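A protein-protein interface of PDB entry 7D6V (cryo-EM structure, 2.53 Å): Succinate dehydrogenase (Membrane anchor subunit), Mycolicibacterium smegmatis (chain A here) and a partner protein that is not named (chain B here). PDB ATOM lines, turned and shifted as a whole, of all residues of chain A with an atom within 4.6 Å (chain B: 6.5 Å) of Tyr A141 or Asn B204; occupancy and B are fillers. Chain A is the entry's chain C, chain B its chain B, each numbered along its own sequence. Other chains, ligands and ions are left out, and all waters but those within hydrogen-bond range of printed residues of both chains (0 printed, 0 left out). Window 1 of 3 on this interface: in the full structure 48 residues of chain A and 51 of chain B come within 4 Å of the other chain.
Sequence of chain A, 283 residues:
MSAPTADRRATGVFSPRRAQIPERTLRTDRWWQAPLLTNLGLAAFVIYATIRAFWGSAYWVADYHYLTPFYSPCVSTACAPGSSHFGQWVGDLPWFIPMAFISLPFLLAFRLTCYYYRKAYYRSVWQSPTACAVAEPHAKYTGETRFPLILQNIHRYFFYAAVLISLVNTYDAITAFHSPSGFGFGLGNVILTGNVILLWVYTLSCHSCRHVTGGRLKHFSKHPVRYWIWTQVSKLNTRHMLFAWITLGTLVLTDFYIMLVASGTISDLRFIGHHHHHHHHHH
ND1 of His B156 lies within hydrogen-bond range of OE2 of Glu A136, 3.2 Å away.
O of Ala A139 lies within hydrogen-bond range of ND1 of His B161 (3.0 Å).
ND2 of Asn B164 lies within hydrogen-bond range of O of Tyr A141.
OH of Tyr A141 sits at hydrogen-bond distance from O of Tyr B202 (2.5 Å).
The side-chain amide nitrogen (ND2) of Asn B204 lies close to the side-chain hydroxyl (OG) of Ser A128, at 3.5 Å.
OD1 of Asn B204 sits at hydrogen-bond distance from OH of Tyr A141.
A ring nitrogen (NE2) of His B161 sits close to the side-chain carboxylate (OE1) of Glu A136 (2.2 Å).
A ring nitrogen (NE2) of His B156 is in hydrogen-bond range of the side-chain amide oxygen (OD1) of Asn B204 (2.5 Å).
The side-chain amide nitrogen of Asn B164 is in hydrogen-bond range of the backbone carbonyl oxygen of Val B157 (3.4 Å).
The side-chain carboxylate (OE1) of Glu B163 sits close to a ring nitrogen (ND1) of His B161 (3.4 Å).
OG1 of Thr B206 is in hydrogen-bond range of OD1 of Asn B204, at 3.5 Å.
N of Ser A128 is in hydrogen-bond range of O of Tyr A122 (2.7 Å).
Among the printed residues, pairs that only touch across the chains: Tyr A122 with Asn B204, Tyr A122 with Thr B206, Ser A128 with His B156, Pro A129 with His B156, Pro A129 with Thr B206, Ala A139 with Glu B163, Lys A140 with His B161, Tyr A141 with His B156, Tyr A141 with Val B157, Tyr A141 with His B161, Thr A142 with Tyr B202, Gly A143 with Gly B201 and Gly A143 with Tyr B202.
Tyr A141 touches six residues of chain B.
Printed residues of chain A within 4 Å of Glu B163: Ala A139 (3.7 Å).
Of the printed residues of chain A, Gly B201 touches Gly A143.
Of chain A, only Tyr A122 (3.6 Å), Ser A128 (3.3 Å) and Tyr A141 (3.0 Å) come within 4 Å of Asn B204.
Printed residues of chain A within 4 Å of Thr B206: Tyr A122 (3.6 Å) and Pro A129 (3.4 Å).
The nearest residue of chain B that does not touch Tyr A141 is Cys B203 (4.1 Å).
The nearest residue of chain A that does not touch Asn B204 is Pro A129 (4.2 Å).
Printed residues of chain B that touch a printed residue of chain A: His B156, Val B157, His B161, Glu B163, Asn B164, Gly B201, Tyr B202, Asn B204 and Thr B206.
Hydrophobic or aromatic side chains of chain B within 4 Å of the printed part of chain A: His B156, Val B157, His B161 and Tyr B202.
Of the 9 printed residues of chain A, 9 touch a printed residue of chain B.
Hydrophobic or aromatic side chains of chain A that line the printed part of chain B: Tyr A122, Pro A129 and Tyr A141.
Among the printed residues, no Asp or Glu carboxylate lies within 4 Å of a Lys or Arg side-chain nitrogen of the other chain.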
ATOM      1  N   TYR A 122      -7.527   8.606 -13.868  1.00  0.00           N
ATOM      2  CA  TYR A 122      -8.267   9.794 -13.458  1.00  0.00           C
ATOM      3  C   TYR A 122      -7.421  10.661 -12.540  1.00  0.00           C
ATOM      4  O   TYR A 122      -7.508  11.891 -12.581  1.00  0.00           O
ATOM      5  CB  TYR A 122      -9.570   9.408 -12.755  1.00  0.00           C
ATOM      6  CG  TYR A 122     -10.664   8.902 -13.661  1.00  0.00           C
ATOM      7  CD1 TYR A 122     -10.738   9.297 -14.987  1.00  0.00           C
ATOM      8  CD2 TYR A 122     -11.633   8.035 -13.184  1.00  0.00           C
ATOM      9  CE1 TYR A 122     -11.735   8.830 -15.810  1.00  0.00           C
ATOM     10  CE2 TYR A 122     -12.632   7.565 -13.998  1.00  0.00           C
ATOM     11  CZ  TYR A 122     -12.679   7.965 -15.309  1.00  0.00           C
ATOM     12  OH  TYR A 122     -13.680   7.496 -16.123  1.00  0.00           O
ATOM     13  N   SER A 128      -8.083  14.462 -11.900  1.00  0.00           N
ATOM     14  CA  SER A 128      -9.388  14.705 -11.300  1.00  0.00           C
ATOM     15  C   SER A 128      -9.185  15.053  -9.827  1.00  0.00           C
ATOM     16  O   SER A 128      -9.406  16.206  -9.463  1.00  0.00           O
ATOM     17  CB  SER A 128     -10.326  13.523 -11.521  1.00  0.00           C
ATOM     18  OG  SER A 128     -10.844  13.542 -12.836  1.00  0.00           O
ATOM     19  N   PRO A 129      -8.770  14.159  -8.944  1.00  0.00           N
ATOM     20  CA  PRO A 129      -7.784  14.610  -7.960  1.00  0.00           C
ATOM     21  C   PRO A 129      -6.390  14.209  -8.413  1.00  0.00           C
ATOM     22  O   PRO A 129      -6.151  13.026  -8.672  1.00  0.00           O
ATOM     23  CB  PRO A 129      -8.219  13.916  -6.666  1.00  0.00           C
ATOM     24  CG  PRO A 129      -8.904  12.712  -7.103  1.00  0.00           C
ATOM     25  CD  PRO A 129      -9.504  12.978  -8.455  1.00  0.00           C
ATOM     26  N   GLU A 136      -8.435  21.076  -7.886  1.00  0.00           N
ATOM     27  CA  GLU A 136      -8.457  20.663  -9.281  1.00  0.00           C
ATOM     28  C   GLU A 136      -7.981  21.769 -10.219  1.00  0.00           C
ATOM     29  O   GLU A 136      -8.230  22.952  -9.979  1.00  0.00           O
ATOM     30  CB  GLU A 136      -9.869  20.270  -9.693  1.00  0.00           C
ATOM     31  CG  GLU A 136     -10.205  18.861  -9.377  1.00  0.00           C
ATOM     32  CD  GLU A 136     -11.613  18.476  -9.764  1.00  0.00           C
ATOM     33  OE1 GLU A 136     -12.557  19.181  -9.368  1.00  0.00           O
ATOM     34  OE2 GLU A 136     -11.777  17.459 -10.464  1.00  0.00           O
ATOM     35  N   ALA A 139     -12.563  23.451 -13.900  1.00  0.00           N
ATOM     36  CA  ALA A 139     -13.626  24.299 -13.375  1.00  0.00           C
ATOM     37  C   ALA A 139     -14.972  23.584 -13.339  1.00  0.00           C
ATOM     38  O   ALA A 139     -15.752  23.779 -12.401  1.00  0.00           O
ATOM     39  CB  ALA A 139     -13.738  25.578 -14.205  1.00  0.00           C
ATOM     40  N   LYS A 140     -15.258  22.760 -14.341  1.00  0.00           N
ATOM     41  CA  LYS A 140     -16.464  21.953 -14.384  1.00  0.00           C
ATOM     42  C   LYS A 140     -16.106  20.483 -14.214  1.00  0.00           C
ATOM     43  O   LYS A 140     -14.988  20.061 -14.519  1.00  0.00           O
ATOM     44  CB  LYS A 140     -17.222  22.158 -15.699  1.00  0.00           C
ATOM     45  CG  LYS A 140     -17.696  23.581 -15.917  1.00  0.00           C
ATOM     46  CD  LYS A 140     -18.765  23.949 -14.907  1.00  0.00           C
ATOM     47  CE  LYS A 140     -19.312  25.341 -15.150  1.00  0.00           C
ATOM     48  NZ  LYS A 140     -20.328  25.705 -14.126  1.00  0.00           N
ATOM     49  N   TYR A 141     -17.063  19.706 -13.714  1.00  0.00           N
ATOM     50  CA  TYR A 141     -16.845  18.280 -13.491  1.00  0.00           C
ATOM     51  C   TYR A 141     -18.183  17.566 -13.532  1.00  0.00           C
ATOM     52  O   TYR A 141     -19.084  17.894 -12.754  1.00  0.00           O
ATOM     53  CB  TYR A 141     -16.149  18.042 -12.157  1.00  0.00           C
ATOM     54  CG  TYR A 141     -16.084  16.594 -11.739  1.00  0.00           C
ATOM     55  CD1 TYR A 141     -15.108  15.748 -12.240  1.00  0.00           C
ATOM     56  CD2 TYR A 141     -16.998  16.076 -10.837  1.00  0.00           C
ATOM     57  CE1 TYR A 141     -15.050  14.428 -11.858  1.00  0.00           C
ATOM     58  CE2 TYR A 141     -16.949  14.761 -10.452  1.00  0.00           C
ATOM     59  CZ  TYR A 141     -15.973  13.942 -10.963  1.00  0.00           C
ATOM     60  OH  TYR A 141     -15.926  12.626 -10.573  1.00  0.00           O
ATOM     61  N   THR A 142     -18.315  16.590 -14.428  1.00  0.00           N
ATOM     62  CA  THR A 142     -19.509  15.766 -14.497  1.00  0.00           C
ATOM     63  C   THR A 142     -19.277  14.333 -14.043  1.00  0.00           C
ATOM     64  O   THR A 142     -20.252  13.619 -13.792  1.00  0.00           O
ATOM     65  CB  THR A 142     -20.078  15.762 -15.923  1.00  0.00           C
ATOM     66  OG1 THR A 142     -19.211  15.020 -16.789  1.00  0.00           O
ATOM     67  CG2 THR A 142     -20.218  17.176 -16.439  1.00  0.00           C
ATOM     68  N   GLY A 143     -18.033  13.900 -13.922  1.00  0.00           N
ATOM     69  CA  GLY A 143     -17.767  12.545 -13.474  1.00  0.00           C
ATOM     70  C   GLY A 143     -17.996  11.553 -14.586  1.00  0.00           C
ATOM     71  O   GLY A 143     -17.497  11.722 -15.698  1.00  0.00           O
ATOM     72  N   HIS B 156     -13.455  15.301  -4.108  1.00  0.00           N
ATOM     73  CA  HIS B 156     -13.254  16.415  -5.027  1.00  0.00           C
ATOM     74  C   HIS B 156     -14.521  16.808  -5.769  1.00  0.00           C
ATOM     75  O   HIS B 156     -14.566  17.899  -6.343  1.00  0.00           O
ATOM     76  CB  HIS B 156     -12.164  16.072  -6.041  1.00  0.00           C
ATOM     77  CG  HIS B 156     -12.563  15.013  -7.019  1.00  0.00           C
ATOM     78  ND1 HIS B 156     -12.695  15.260  -8.369  1.00  0.00           N
ATOM     79  CD2 HIS B 156     -12.872  13.706  -6.843  1.00  0.00           C
ATOM     80  CE1 HIS B 156     -13.062  14.150  -8.981  1.00  0.00           C
ATOM     81  NE2 HIS B 156     -13.175  13.194  -8.079  1.00  0.00           N
ATOM     82  N   VAL B 157     -15.541  15.948  -5.782  1.00  0.00           N
ATOM     83  CA  VAL B 157     -16.776  16.272  -6.487  1.00  0.00           C
ATOM     84  C   VAL B 157     -17.402  17.532  -5.908  1.00  0.00           C
ATOM     85  O   VAL B 157     -17.832  18.426  -6.645  1.00  0.00           O
ATOM     86  CB  VAL B 157     -17.751  15.081  -6.437  1.00  0.00           C
ATOM     87  CG1 VAL B 157     -19.028  15.410  -7.185  1.00  0.00           C
ATOM     88  CG2 VAL B 157     -17.101  13.843  -7.012  1.00  0.00           C
ATOM     89  N   VAL B 158     -17.451  17.629  -4.583  1.00  0.00           N
ATOM     90  CA  VAL B 158     -18.007  18.798  -3.918  1.00  0.00           C
ATOM     91  C   VAL B 158     -16.937  19.712  -3.335  1.00  0.00           C
ATOM     92  O   VAL B 158     -17.202  20.912  -3.165  1.00  0.00           O
ATOM     93  CB  VAL B 158     -19.013  18.390  -2.822  1.00  0.00           C
ATOM     94  CG1 VAL B 158     -20.293  17.880  -3.450  1.00  0.00           C
ATOM     95  CG2 VAL B 158     -18.409  17.334  -1.921  1.00  0.00           C
ATOM     96  N   HIS B 161     -15.970  21.811  -6.458  1.00  0.00           N
ATOM     97  CA  HIS B 161     -17.074  22.274  -7.296  1.00  0.00           C
ATOM     98  C   HIS B 161     -18.279  22.542  -6.409  1.00  0.00           C
ATOM     99  O   HIS B 161     -18.898  21.604  -5.899  1.00  0.00           O
ATOM    100  CB  HIS B 161     -17.405  21.252  -8.380  1.00  0.00           C
ATOM    101  CG  HIS B 161     -16.233  20.892  -9.234  1.00  0.00           C
ATOM    102  ND1 HIS B 161     -15.792  21.691 -10.267  1.00  0.00           N
ATOM    103  CD2 HIS B 161     -15.390  19.837  -9.189  1.00  0.00           C
ATOM    104  CE1 HIS B 161     -14.736  21.135 -10.830  1.00  0.00           C
ATOM    105  NE2 HIS B 161     -14.470  20.009 -10.193  1.00  0.00           N
ATOM    106  N   GLU B 163     -21.087  23.875  -7.403  1.00  0.00           N
ATOM    107  CA  GLU B 163     -22.320  23.624  -8.137  1.00  0.00           C
ATOM    108  C   GLU B 163     -22.773  22.174  -8.037  1.00  0.00           C
ATOM    109  O   GLU B 163     -23.945  21.886  -8.298  1.00  0.00           O
ATOM    110  CB  GLU B 163     -22.143  24.012  -9.604  1.00  0.00           C
ATOM    111  CG  GLU B 163     -21.248  23.074 -10.396  1.00  0.00           C
ATOM    112  CD  GLU B 163     -19.784  23.462 -10.328  1.00  0.00           C
ATOM    113  OE1 GLU B 163     -18.943  22.711 -10.864  1.00  0.00           O
ATOM    114  OE2 GLU B 163     -19.473  24.517  -9.740  1.00  0.00           O
ATOM    115  N   ASN B 164     -21.883  21.264  -7.663  1.00  0.00           N
ATOM    116  CA  ASN B 164     -22.205  19.849  -7.553  1.00  0.00           C
ATOM    117  C   ASN B 164     -22.772  19.474  -6.192  1.00  0.00           C
ATOM    118  O   ASN B 164     -23.093  18.304  -5.975  1.00  0.00           O
ATOM    119  CB  ASN B 164     -20.962  19.004  -7.839  1.00  0.00           C
ATOM    120  CG  ASN B 164     -20.629  18.938  -9.311  1.00  0.00           C
ATOM    121  OD1 ASN B 164     -21.466  19.230 -10.162  1.00  0.00           O
ATOM    122  ND2 ASN B 164     -19.402  18.550  -9.621  1.00  0.00           N
ATOM    123  N   LEU B 200     -24.840   9.221  -8.061  1.00  0.00           N
ATOM    124  CA  LEU B 200     -23.767   8.238  -7.952  1.00  0.00           C
ATOM    125  C   LEU B 200     -22.831   8.287  -9.154  1.00  0.00           C
ATOM    126  O   LEU B 200     -21.661   7.907  -9.045  1.00  0.00           O
ATOM    127  CB  LEU B 200     -24.354   6.838  -7.787  1.00  0.00           C
ATOM    128  CG  LEU B 200     -23.385   5.683  -7.531  1.00  0.00           C
ATOM    129  CD1 LEU B 200     -22.491   5.975  -6.342  1.00  0.00           C
ATOM    130  CD2 LEU B 200     -24.149   4.394  -7.325  1.00  0.00           C
ATOM    131  N   GLY B 201     -23.317   8.760 -10.303  1.00  0.00           N
ATOM    132  CA  GLY B 201     -22.471   8.866 -11.477  1.00  0.00           C
ATOM    133  C   GLY B 201     -21.394   9.922 -11.370  1.00  0.00           C
ATOM    134  O   GLY B 201     -20.389   9.839 -12.081  1.00  0.00           O
ATOM    135  N   TYR B 202     -21.582  10.917 -10.500  1.00  0.00           N
ATOM    136  CA  TYR B 202     -20.564  11.944 -10.314  1.00  0.00           C
ATOM    137  C   TYR B 202     -19.299  11.375  -9.697  1.00  0.00           C
ATOM    138  O   TYR B 202     -18.216  11.940  -9.876  1.00  0.00           O
ATOM    139  CB  TYR B 202     -21.109  13.074  -9.446  1.00  0.00           C
ATOM    140  CG  TYR B 202     -21.968  14.050 -10.204  1.00  0.00           C
ATOM    141  CD1 TYR B 202     -23.345  13.910 -10.236  1.00  0.00           C
ATOM    142  CD2 TYR B 202     -21.402  15.110 -10.892  1.00  0.00           C
ATOM    143  CE1 TYR B 202     -24.130  14.796 -10.931  1.00  0.00           C
ATOM    144  CE2 TYR B 202     -22.179  16.002 -11.587  1.00  0.00           C
ATOM    145  CZ  TYR B 202     -23.542  15.841 -11.604  1.00  0.00           C
ATOM    146  OH  TYR B 202     -24.323  16.730 -12.299  1.00  0.00           O
ATOM    147  N   CYS B 203     -19.595  10.309  -9.010  1.00  0.00           N
ATOM    148  CA  CYS B 203     -18.444   9.681  -8.377  1.00  0.00           C
ATOM    149  C   CYS B 203     -17.584   8.999  -9.429  1.00  0.00           C
ATOM    150  O   CYS B 203     -17.971   7.969  -9.986  1.00  0.00           O
ATOM    151  CB  CYS B 203     -18.897   8.677  -7.322  1.00  0.00           C
ATOM    152  SG  CYS B 203     -17.547   7.837  -6.462  1.00  0.00           S
ATOM    153  N   ASN B 204     -16.244   9.536  -9.688  1.00  0.00           N
ATOM    154  CA  ASN B 204     -15.138   8.739 -10.179  1.00  0.00           C
ATOM    155  C   ASN B 204     -14.420   8.182  -8.961  1.00  0.00           C
ATOM    156  O   ASN B 204     -14.414   8.797  -7.894  1.00  0.00           O
ATOM    157  CB  ASN B 204     -14.207   9.555 -11.083  1.00  0.00           C
ATOM    158  CG  ASN B 204     -13.380  10.578 -10.333  1.00  0.00           C
ATOM    159  OD1 ASN B 204     -13.735  11.017  -9.246  1.00  0.00           O
ATOM    160  ND2 ASN B 204     -12.271  10.976 -10.931  1.00  0.00           N
ATOM    161  N   ILE B 205     -13.824   7.012  -9.113  1.00  0.00           N
ATOM    162  CA  ILE B 205     -13.561   6.156  -7.963  1.00  0.00           C
ATOM    163  C   ILE B 205     -12.134   6.324  -7.467  1.00  0.00           C
ATOM    164  O   ILE B 205     -11.520   5.380  -6.957  1.00  0.00           O
ATOM    165  CB  ILE B 205     -13.886   4.695  -8.293  1.00  0.00           C
ATOM    166  CG1 ILE B 205     -12.999   4.210  -9.427  1.00  0.00           C
ATOM    167  CG2 ILE B 205     -15.351   4.543  -8.646  1.00  0.00           C
ATOM    168  CD1 ILE B 205     -13.111   2.777  -9.619  1.00  0.00           C
ATOM    169  N   THR B 206     -11.595   7.528  -7.632  1.00  0.00           N
ATOM    170  CA  THR B 206     -10.223   7.862  -7.273  1.00  0.00           C
ATOM    171  C   THR B 206      -9.872   7.599  -5.809  1.00  0.00           C
ATOM    172  O   THR B 206      -8.701   7.683  -5.433  1.00  0.00           O
ATOM    173  CB  THR B 206      -9.960   9.320  -7.625  1.00  0.00           C
ATOM    174  OG1 THR B 206     -11.082  10.113  -7.221  1.00  0.00           O
ATOM    175  CG2 THR B 206      -9.774   9.453  -9.118  1.00  0.00           C
ATOM    176  N   LYS B 207     -10.872   7.316  -4.973  1.00  0.00           N
ATOM    177  CA  LYS B 207     -10.699   6.624  -3.696  1.00  0.00           C
ATOM    178  C   LYS B 207     -10.049   7.475  -2.606  1.00  0.00           C
ATOM    179  O   LYS B 207      -9.629   6.938  -1.582  1.00  0.00           O
ATOM    180  CB  LYS B 207      -9.894   5.330  -3.891  1.00  0.00           C
ATOM    181  CG  LYS B 207     -10.276   4.191  -2.969  1.00  0.00           C
ATOM    182  CD  LYS B 207      -9.229   3.091  -2.970  1.00  0.00           C
ATOM    183  CE  LYS B 207      -9.429   2.134  -4.128  1.00  0.00           C
ATOM    184  NZ  LYS B 207     -10.626   1.270  -3.943  1.00  0.00           N
ATOM    185  N   THR B 220     -14.967   2.833  -0.912  1.00  0.00           N
ATOM    186  CA  THR B 220     -15.042   2.669  -2.358  1.00  0.00           C
ATOM    187  C   THR B 220     -15.242   1.209  -2.746  1.00  0.00           C
ATOM    188  O   THR B 220     -16.095   0.891  -3.582  1.00  0.00           O
ATOM    189  CB  THR B 220     -13.785   3.234  -3.014  1.00  0.00           C
ATOM    190  OG1 THR B 220     -13.511   4.530  -2.473  1.00  0.00           O
ATOM    191  CG2 THR B 220     -13.976   3.358  -4.511  1.00  0.00           C
ATOM    192  N   LYS B 228     -22.487   0.882  -7.788  1.00  0.00           N
ATOM    193  CA  LYS B 228     -22.382   1.191  -9.210  1.00  0.00           C
ATOM    194  C   LYS B 228     -22.691  -0.036 -10.057  1.00  0.00           C
ATOM    195  O   LYS B 228     -23.341   0.069 -11.100  1.00  0.00           O
ATOM    196  CB  LYS B 228     -20.993   1.735  -9.531  1.00  0.00           C
ATOM    197  CG  LYS B 228     -20.799   3.186  -9.147  1.00  0.00           C
ATOM    198  CD  LYS B 228     -19.358   3.614  -9.315  1.00  0.00           C
ATOM    199  CE  LYS B 228     -19.186   5.098  -9.040  1.00  0.00           C
ATOM    200  NZ  LYS B 228     -19.480   5.937 -10.230  1.00  0.00           N
